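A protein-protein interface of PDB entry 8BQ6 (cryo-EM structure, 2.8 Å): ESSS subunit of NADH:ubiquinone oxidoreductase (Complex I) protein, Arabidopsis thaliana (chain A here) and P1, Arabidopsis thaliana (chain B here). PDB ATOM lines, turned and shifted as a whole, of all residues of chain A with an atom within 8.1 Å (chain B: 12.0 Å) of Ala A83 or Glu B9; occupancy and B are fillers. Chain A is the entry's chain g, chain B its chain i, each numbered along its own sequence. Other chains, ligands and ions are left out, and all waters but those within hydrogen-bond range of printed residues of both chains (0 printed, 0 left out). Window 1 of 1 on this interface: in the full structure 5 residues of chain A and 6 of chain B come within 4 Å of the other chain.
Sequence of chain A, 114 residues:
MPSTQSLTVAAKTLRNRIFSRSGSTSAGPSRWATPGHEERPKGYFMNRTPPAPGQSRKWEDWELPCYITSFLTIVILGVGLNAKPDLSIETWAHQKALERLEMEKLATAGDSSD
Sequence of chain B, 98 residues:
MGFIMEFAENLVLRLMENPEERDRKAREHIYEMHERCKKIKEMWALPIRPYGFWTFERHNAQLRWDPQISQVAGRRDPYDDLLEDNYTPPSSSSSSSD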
ATOM      1  N   ILE A  76      26.568  17.196  27.874  1.00  0.00           N
ATOM      2  CA  ILE A  76      25.498  17.361  26.891  1.00  0.00           C
ATOM      3  C   ILE A  76      24.272  16.550  27.292  1.00  0.00           C
ATOM      4  O   ILE A  76      23.144  17.054  27.289  1.00  0.00           O
ATOM      5  CB  ILE A  76      25.992  16.982  25.484  1.00  0.00           C
ATOM      6  CG1 ILE A  76      26.816  18.119  24.891  1.00  0.00           C
ATOM      7  CG2 ILE A  76      24.821  16.675  24.572  1.00  0.00           C
ATOM      8  CD1 ILE A  76      27.620  17.707  23.688  1.00  0.00           C
ATOM      9  N   LEU A  77      24.472  15.280  27.645  1.00  0.00           N
ATOM     10  CA  LEU A  77      23.342  14.418  27.978  1.00  0.00           C
ATOM     11  C   LEU A  77      22.802  14.722  29.373  1.00  0.00           C
ATOM     12  O   LEU A  77      21.597  14.613  29.620  1.00  0.00           O
ATOM     13  CB  LEU A  77      23.756  12.952  27.871  1.00  0.00           C
ATOM     14  CG  LEU A  77      24.058  12.414  26.472  1.00  0.00           C
ATOM     15  CD1 LEU A  77      24.403  10.936  26.538  1.00  0.00           C
ATOM     16  CD2 LEU A  77      22.897  12.660  25.523  1.00  0.00           C
ATOM     17  N   GLY A  78      23.685  15.079  30.307  1.00  0.00           N
ATOM     18  CA  GLY A  78      23.229  15.413  31.647  1.00  0.00           C
ATOM     19  C   GLY A  78      22.433  16.701  31.699  1.00  0.00           C
ATOM     20  O   GLY A  78      21.463  16.808  32.453  1.00  0.00           O
ATOM     21  N   VAL A  79      22.832  17.692  30.908  1.00  0.00           N
ATOM     22  CA  VAL A  79      22.129  18.968  30.853  1.00  0.00           C
ATOM     23  C   VAL A  79      21.050  18.956  29.782  1.00  0.00           C
ATOM     24  O   VAL A  79      19.899  19.314  30.042  1.00  0.00           O
ATOM     25  CB  VAL A  79      23.142  20.112  30.623  1.00  0.00           C
ATOM     26  CG1 VAL A  79      22.486  21.292  29.910  1.00  0.00           C
ATOM     27  CG2 VAL A  79      23.760  20.546  31.935  1.00  0.00           C
ATOM     28  N   GLY A  80      21.399  18.525  28.568  1.00  0.00           N
ATOM     29  CA  GLY A  80      20.463  18.625  27.461  1.00  0.00           C
ATOM     30  C   GLY A  80      19.202  17.809  27.665  1.00  0.00           C
ATOM     31  O   GLY A  80      18.098  18.277  27.374  1.00  0.00           O
ATOM     32  N   LEU A  81      19.343  16.583  28.166  1.00  0.00           N
ATOM     33  CA  LEU A  81      18.173  15.727  28.334  1.00  0.00           C
ATOM     34  C   LEU A  81      17.270  16.245  29.445  1.00  0.00           C
ATOM     35  O   LEU A  81      16.040  16.149  29.350  1.00  0.00           O
ATOM     36  CB  LEU A  81      18.617  14.292  28.607  1.00  0.00           C
ATOM     37  CG  LEU A  81      19.229  13.601  27.385  1.00  0.00           C
ATOM     38  CD1 LEU A  81      19.640  12.183  27.718  1.00  0.00           C
ATOM     39  CD2 LEU A  81      18.272  13.618  26.208  1.00  0.00           C
ATOM     40  N   ASN A  82      17.858  16.813  30.497  1.00  0.00           N
ATOM     41  CA  ASN A  82      17.093  17.421  31.576  1.00  0.00           C
ATOM     42  C   ASN A  82      16.653  18.846  31.272  1.00  0.00           C
ATOM     43  O   ASN A  82      15.899  19.424  32.061  1.00  0.00           O
ATOM     44  CB  ASN A  82      17.911  17.398  32.868  1.00  0.00           C
ATOM     45  CG  ASN A  82      18.046  16.006  33.439  1.00  0.00           C
ATOM     46  OD1 ASN A  82      17.112  15.482  34.045  1.00  0.00           O
ATOM     47  ND2 ASN A  82      19.204  15.392  33.241  1.00  0.00           N
ATOM     48  N   ALA A  83      17.097  19.428  30.156  1.00  0.00           N
ATOM     49  CA  ALA A  83      16.696  20.778  29.789  1.00  0.00           C
ATOM     50  C   ALA A  83      15.813  20.832  28.554  1.00  0.00           C
ATOM     51  O   ALA A  83      15.140  21.843  28.341  1.00  0.00           O
ATOM     52  CB  ALA A  83      17.924  21.659  29.549  1.00  0.00           C
ATOM     53  N   LYS A  84      15.812  19.796  27.726  1.00  0.00           N
ATOM     54  CA  LYS A  84      14.866  19.768  26.632  1.00  0.00           C
ATOM     55  C   LYS A  84      13.451  19.649  27.194  1.00  0.00           C
ATOM     56  O   LYS A  84      13.243  19.046  28.250  1.00  0.00           O
ATOM     57  CB  LYS A  84      15.169  18.615  25.677  1.00  0.00           C
ATOM     58  CG  LYS A  84      15.088  17.236  26.296  1.00  0.00           C
ATOM     59  CD  LYS A  84      15.460  16.150  25.297  1.00  0.00           C
ATOM     60  CE  LYS A  84      15.004  16.490  23.889  1.00  0.00           C
ATOM     61  NZ  LYS A  84      14.637  15.265  23.133  1.00  0.00           N
ATOM     62  N   PRO A  85      12.469  20.263  26.539  1.00  0.00           N
ATOM     63  CA  PRO A  85      11.097  20.190  27.045  1.00  0.00           C
ATOM     64  C   PRO A  85      10.544  18.776  26.944  1.00  0.00           C
ATOM     65  O   PRO A  85      10.959  17.978  26.103  1.00  0.00           O
ATOM     66  CB  PRO A  85      10.333  21.159  26.139  1.00  0.00           C
ATOM     67  CG  PRO A  85      11.140  21.200  24.877  1.00  0.00           C
ATOM     68  CD  PRO A  85      12.568  21.075  25.314  1.00  0.00           C
ATOM     69  N   ASP A  86       9.606  18.465  27.833  1.00  0.00           N
ATOM     70  CA  ASP A  86       8.915  17.182  27.788  1.00  0.00           C
ATOM     71  C   ASP A  86       7.838  17.259  26.714  1.00  0.00           C
ATOM     72  O   ASP A  86       6.794  17.888  26.917  1.00  0.00           O
ATOM     73  CB  ASP A  86       8.317  16.847  29.150  1.00  0.00           C
ATOM     74  CG  ASP A  86       7.798  15.423  29.229  1.00  0.00           C
ATOM     75  OD1 ASP A  86       7.643  14.915  30.357  1.00  0.00           O
ATOM     76  OD2 ASP A  86       7.540  14.810  28.173  1.00  0.00           O
ATOM     77  N   GLY B   2      21.768  33.443  34.215  1.00  0.00           N
ATOM     78  CA  GLY B   2      22.353  33.190  35.518  1.00  0.00           C
ATOM     79  C   GLY B   2      22.244  31.732  35.909  1.00  0.00           C
ATOM     80  O   GLY B   2      23.253  31.044  36.074  1.00  0.00           O
ATOM     81  N   PHE B   3      21.006  31.264  36.057  1.00  0.00           N
ATOM     82  CA  PHE B   3      20.764  29.858  36.335  1.00  0.00           C
ATOM     83  C   PHE B   3      21.170  29.009  35.135  1.00  0.00           C
ATOM     84  O   PHE B   3      20.898  29.351  33.980  1.00  0.00           O
ATOM     85  CB  PHE B   3      19.288  29.633  36.680  1.00  0.00           C
ATOM     86  CG  PHE B   3      19.019  28.337  37.389  1.00  0.00           C
ATOM     87  CD1 PHE B   3      17.750  27.780  37.393  1.00  0.00           C
ATOM     88  CD2 PHE B   3      20.034  27.677  38.059  1.00  0.00           C
ATOM     89  CE1 PHE B   3      17.503  26.588  38.051  1.00  0.00           C
ATOM     90  CE2 PHE B   3      19.794  26.486  38.714  1.00  0.00           C
ATOM     91  CZ  PHE B   3      18.530  25.940  38.710  1.00  0.00           C
ATOM     92  N   ILE B   4      21.844  27.895  35.419  1.00  0.00           N
ATOM     93  CA  ILE B   4      22.323  27.021  34.353  1.00  0.00           C
ATOM     94  C   ILE B   4      21.149  26.410  33.598  1.00  0.00           C
ATOM     95  O   ILE B   4      21.086  26.462  32.364  1.00  0.00           O
ATOM     96  CB  ILE B   4      23.257  25.940  34.929  1.00  0.00           C
ATOM     97  CG1 ILE B   4      24.702  26.439  34.971  1.00  0.00           C
ATOM     98  CG2 ILE B   4      23.178  24.649  34.119  1.00  0.00           C
ATOM     99  CD1 ILE B   4      24.964  27.498  36.012  1.00  0.00           C
ATOM    100  N   MET B   5      20.185  25.851  34.330  1.00  0.00           N
ATOM    101  CA  MET B   5      19.113  25.106  33.681  1.00  0.00           C
ATOM    102  C   MET B   5      18.226  26.014  32.838  1.00  0.00           C
ATOM    103  O   MET B   5      17.927  25.686  31.685  1.00  0.00           O
ATOM    104  CB  MET B   5      18.301  24.342  34.726  1.00  0.00           C
ATOM    105  CG  MET B   5      19.023  23.104  35.237  1.00  0.00           C
ATOM    106  SD  MET B   5      20.117  22.413  33.973  1.00  0.00           S
ATOM    107  CE  MET B   5      19.239  20.923  33.515  1.00  0.00           C
ATOM    108  N   GLU B   6      17.830  27.176  33.371  1.00  0.00           N
ATOM    109  CA  GLU B   6      16.965  28.078  32.611  1.00  0.00           C
ATOM    110  C   GLU B   6      17.646  28.554  31.334  1.00  0.00           C
ATOM    111  O   GLU B   6      16.995  28.696  30.291  1.00  0.00           O
ATOM    112  CB  GLU B   6      16.552  29.274  33.468  1.00  0.00           C
ATOM    113  CG  GLU B   6      15.689  28.926  34.672  1.00  0.00           C
ATOM    114  CD  GLU B   6      14.195  29.052  34.406  1.00  0.00           C
ATOM    115  OE1 GLU B   6      13.768  28.932  33.238  1.00  0.00           O
ATOM    116  OE2 GLU B   6      13.442  29.274  35.379  1.00  0.00           O
ATOM    117  N   PHE B   7      18.949  28.821  31.394  1.00  0.00           N
ATOM    118  CA  PHE B   7      19.685  29.128  30.173  1.00  0.00           C
ATOM    119  C   PHE B   7      19.625  27.953  29.205  1.00  0.00           C
ATOM    120  O   PHE B   7      19.432  28.136  27.997  1.00  0.00           O
ATOM    121  CB  PHE B   7      21.132  29.490  30.508  1.00  0.00           C
ATOM    122  CG  PHE B   7      22.062  29.418  29.334  1.00  0.00           C
ATOM    123  CD1 PHE B   7      22.786  28.267  29.080  1.00  0.00           C
ATOM    124  CD2 PHE B   7      22.205  30.495  28.480  1.00  0.00           C
ATOM    125  CE1 PHE B   7      23.636  28.195  28.003  1.00  0.00           C
ATOM    126  CE2 PHE B   7      23.058  30.429  27.400  1.00  0.00           C
ATOM    127  CZ  PHE B   7      23.774  29.277  27.161  1.00  0.00           C
ATOM    128  N   ALA B   8      19.778  26.734  29.727  1.00  0.00           N
ATOM    129  CA  ALA B   8      19.757  25.546  28.879  1.00  0.00           C
ATOM    130  C   ALA B   8      18.364  25.284  28.321  1.00  0.00           C
ATOM    131  O   ALA B   8      18.225  24.837  27.176  1.00  0.00           O
ATOM    132  CB  ALA B   8      20.263  24.338  29.664  1.00  0.00           C
ATOM    133  N   GLU B   9      17.321  25.544  29.114  1.00  0.00           N
ATOM    134  CA  GLU B   9      15.956  25.429  28.608  1.00  0.00           C
ATOM    135  C   GLU B   9      15.763  26.288  27.362  1.00  0.00           C
ATOM    136  O   GLU B   9      15.282  25.808  26.331  1.00  0.00           O
ATOM    137  CB  GLU B   9      14.952  25.822  29.698  1.00  0.00           C
ATOM    138  CG  GLU B   9      15.085  25.029  30.999  1.00  0.00           C
ATOM    139  CD  GLU B   9      14.264  23.751  31.031  1.00  0.00           C
ATOM    140  OE1 GLU B   9      14.107  23.177  32.129  1.00  0.00           O
ATOM    141  OE2 GLU B   9      13.742  23.340  29.977  1.00  0.00           O
ATOM    142  N   ASN B  10      16.151  27.564  27.436  1.00  0.00           N
ATOM    143  CA  ASN B  10      16.066  28.433  26.265  1.00  0.00           C
ATOM    144  C   ASN B  10      16.976  27.949  25.147  1.00  0.00           C
ATOM    145  O   ASN B  10      16.586  27.951  23.973  1.00  0.00           O
ATOM    146  CB  ASN B  10      16.430  29.866  26.640  1.00  0.00           C
ATOM    147  CG  ASN B  10      15.746  30.325  27.898  1.00  0.00           C
ATOM    148  OD1 ASN B  10      14.553  30.095  28.091  1.00  0.00           O
ATOM    149  ND2 ASN B  10      16.501  30.976  28.774  1.00  0.00           N
ATOM    150  N   LEU B  11      18.202  27.546  25.491  1.00  0.00           N
ATOM    151  CA  LEU B  11      19.165  27.162  24.467  1.00  0.00           C
ATOM    152  C   LEU B  11      18.669  25.972  23.654  1.00  0.00           C
ATOM    153  O   LEU B  11      18.785  25.963  22.424  1.00  0.00           O
ATOM    154  CB  LEU B  11      20.516  26.847  25.104  1.00  0.00           C
ATOM    155  CG  LEU B  11      21.578  26.418  24.090  1.00  0.00           C
ATOM    156  CD1 LEU B  11      21.643  27.399  22.930  1.00  0.00           C
ATOM    157  CD2 LEU B  11      22.935  26.267  24.747  1.00  0.00           C
ATOM    158  N   VAL B  12      18.115  24.957  24.320  1.00  0.00           N
ATOM    159  CA  VAL B  12      17.552  23.832  23.581  1.00  0.00           C
ATOM    160  C   VAL B  12      16.340  24.276  22.773  1.00  0.00           C
ATOM    161  O   VAL B  12      16.171  23.877  21.616  1.00  0.00           O
ATOM    162  CB  VAL B  12      17.204  22.671  24.529  1.00  0.00           C
ATOM    163  CG1 VAL B  12      16.694  21.496  23.726  1.00  0.00           C
ATOM    164  CG2 VAL B  12      18.424  22.253  25.326  1.00  0.00           C
ATOM    165  N   LEU B  13      15.477  25.105  23.369  1.00  0.00           N
ATOM    166  CA  LEU B  13      14.291  25.583  22.660  1.00  0.00           C
ATOM    167  C   LEU B  13      14.671  26.350  21.401  1.00  0.00           C
ATOM    168  O   LEU B  13      13.963  26.288  20.389  1.00  0.00           O
ATOM    169  CB  LEU B  13      13.447  26.463  23.579  1.00  0.00           C
ATOM    170  CG  LEU B  13      12.493  25.805  24.574  1.00  0.00           C
ATOM    171  CD1 LEU B  13      11.500  26.831  25.066  1.00  0.00           C
ATOM    172  CD2 LEU B  13      11.769  24.640  23.932  1.00  0.00           C
ATOM    173  N   ARG B  14      15.805  27.054  21.442  1.00  0.00           N
ATOM    174  CA  ARG B  14      16.286  27.801  20.251  1.00  0.00           C
ATOM    175  C   ARG B  14      16.774  26.821  19.182  1.00  0.00           C
ATOM    176  O   ARG B  14      16.693  27.170  17.987  1.00  0.00           O
ATOM    177  CB  ARG B  14      17.437  28.730  20.646  1.00  0.00           C
ATOM    178  CG  ARG B  14      17.435  30.068  19.923  1.00  0.00           C
ATOM    179  CD  ARG B  14      17.999  31.167  20.801  1.00  0.00           C
ATOM    180  NE  ARG B  14      17.021  31.645  21.768  1.00  0.00           N
ATOM    181  CZ  ARG B  14      17.132  31.522  23.087  1.00  0.00           C
ATOM    182  NH1 ARG B  14      18.189  30.929  23.615  1.00  0.00           N
ATOM    183  NH2 ARG B  14      16.182  31.995  23.871  1.00  0.00           N
ATOM    184  N   LEU B  15      17.251  25.642  19.589  1.00  0.00           N
ATOM    185  CA  LEU B  15      17.822  24.696  18.637  1.00  0.00           C
ATOM    186  C   LEU B  15      16.769  23.858  17.924  1.00  0.00           C
ATOM    187  O   LEU B  15      17.015  23.410  16.801  1.00  0.00           O
ATOM    188  CB  LEU B  15      18.813  23.781  19.353  1.00  0.00           C
ATOM    189  CG  LEU B  15      20.142  24.394  19.792  1.00  0.00           C
ATOM    190  CD1 LEU B  15      20.863  23.437  20.716  1.00  0.00           C
ATOM    191  CD2 LEU B  15      21.000  24.717  18.586  1.00  0.00           C
ATOM    192  N   MET B  16      15.614  23.626  18.546  1.00  0.00           N
ATOM    193  CA  MET B  16      14.591  22.786  17.938  1.00  0.00           C
ATOM    194  C   MET B  16      13.958  23.491  16.744  1.00  0.00           C
ATOM    195  O   MET B  16      13.858  24.719  16.711  1.00  0.00           O
ATOM    196  CB  MET B  16      13.513  22.431  18.962  1.00  0.00           C
ATOM    197  CG  MET B  16      14.043  22.131  20.347  1.00  0.00           C
ATOM    198  SD  MET B  16      12.844  21.309  21.409  1.00  0.00           S
ATOM    199  CE  MET B  16      13.793  19.898  21.967  1.00  0.00           C
ATOM    200  N   GLU B  17      13.530  22.708  15.758  1.00  0.00           N
ATOM    201  CA  GLU B  17      12.865  23.288  14.603  1.00  0.00           C
ATOM    202  C   GLU B  17      11.431  23.674  14.962  1.00  0.00           C
ATOM    203  O   GLU B  17      10.832  23.152  15.905  1.00  0.00           O
ATOM    204  CB  GLU B  17      12.895  22.319  13.417  1.00  0.00           C
ATOM    205  CG  GLU B  17      12.330  20.939  13.701  1.00  0.00           C
ATOM    206  CD  GLU B  17      12.635  19.938  12.596  1.00  0.00           C
ATOM    207  OE1 GLU B  17      12.786  20.356  11.428  1.00  0.00           O
ATOM    208  OE2 GLU B  17      12.717  18.730  12.900  1.00  0.00           O
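Among the printed residues, merely in contact across the chains: Ala A83 with Ala B8 (3.6 Å), Pro A85 with Leu B13 (3.6 Å), Pro A85 with Met B16 (3.8 Å), Val A79 with Ala B8 (3.8 Å), Lys A84 with Val B12 (3.8 Å), Asn A82 with Met B5 (3.8 Å) and Val A79 with Met B5 (3.9 Å).
Hydrophobic or aromatic side chains of chain B within 4 Å of the printed part of chain A: Met B5, Ala B8, Val B12, Leu B13 and Met B16. Among the printed residues, 8 pairs touch across the chains. Among the printed residues, no Asp or Glu carboxylate lies within 4 Å of a Lys or Arg side-chain nitrogen of the other chain.
The backbone carbonyl oxygen (O) of Ala A83 sits close to the side-chain carboxylate (OE2) of Glu B9, 2.6 Å away.
Of chain B, only Ala B8 (3.6 Å) and Glu B9 (2.6 Å) come within 4 Å of Ala A83. Of the printed residues of chain A, Glu B9 touches Ala A83 (2.6 Å). No residue of chain B comes within 4 Å of Gly A78. Of chain B, only Met B5 and Ala B8 come within 4 Å of Val A79. Lys A84 touches just one residue of chain B: Val B12. Pro A85 touches just these residues of chain B: Leu B13 and Met B16. Of chain A, only Val A79 and Ala A83 come within 4 Å of Ala B8. Printed residues of chain A within 4 Å of Val B12: Lys A84 (3.8 Å). Printed residues of chain A within 4 Å of Leu B13: Pro A85 (3.6 Å). Printed residues of chain A within 4 Å of Met B16: Pro A85. Asn B10 touches none of the printed residues of chain A. Asp A86 touches none of the printed residues of chain B. The nearest residue of chain B that does not touch Ala A83 is Met B5 (4.2 Å). The nearest residue of chain A that does not touch Glu B9 is Asn A82 (4.2 Å). The nearest printed residue of chain A that does not touch Val B12 is Ala A83 (4.3 Å).
The backbone carbonyl oxygen (O) of Gly A78 is in hydrogen-bond range of the side-chain amide nitrogen (ND2) of Asn A82 (2.8 Å).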
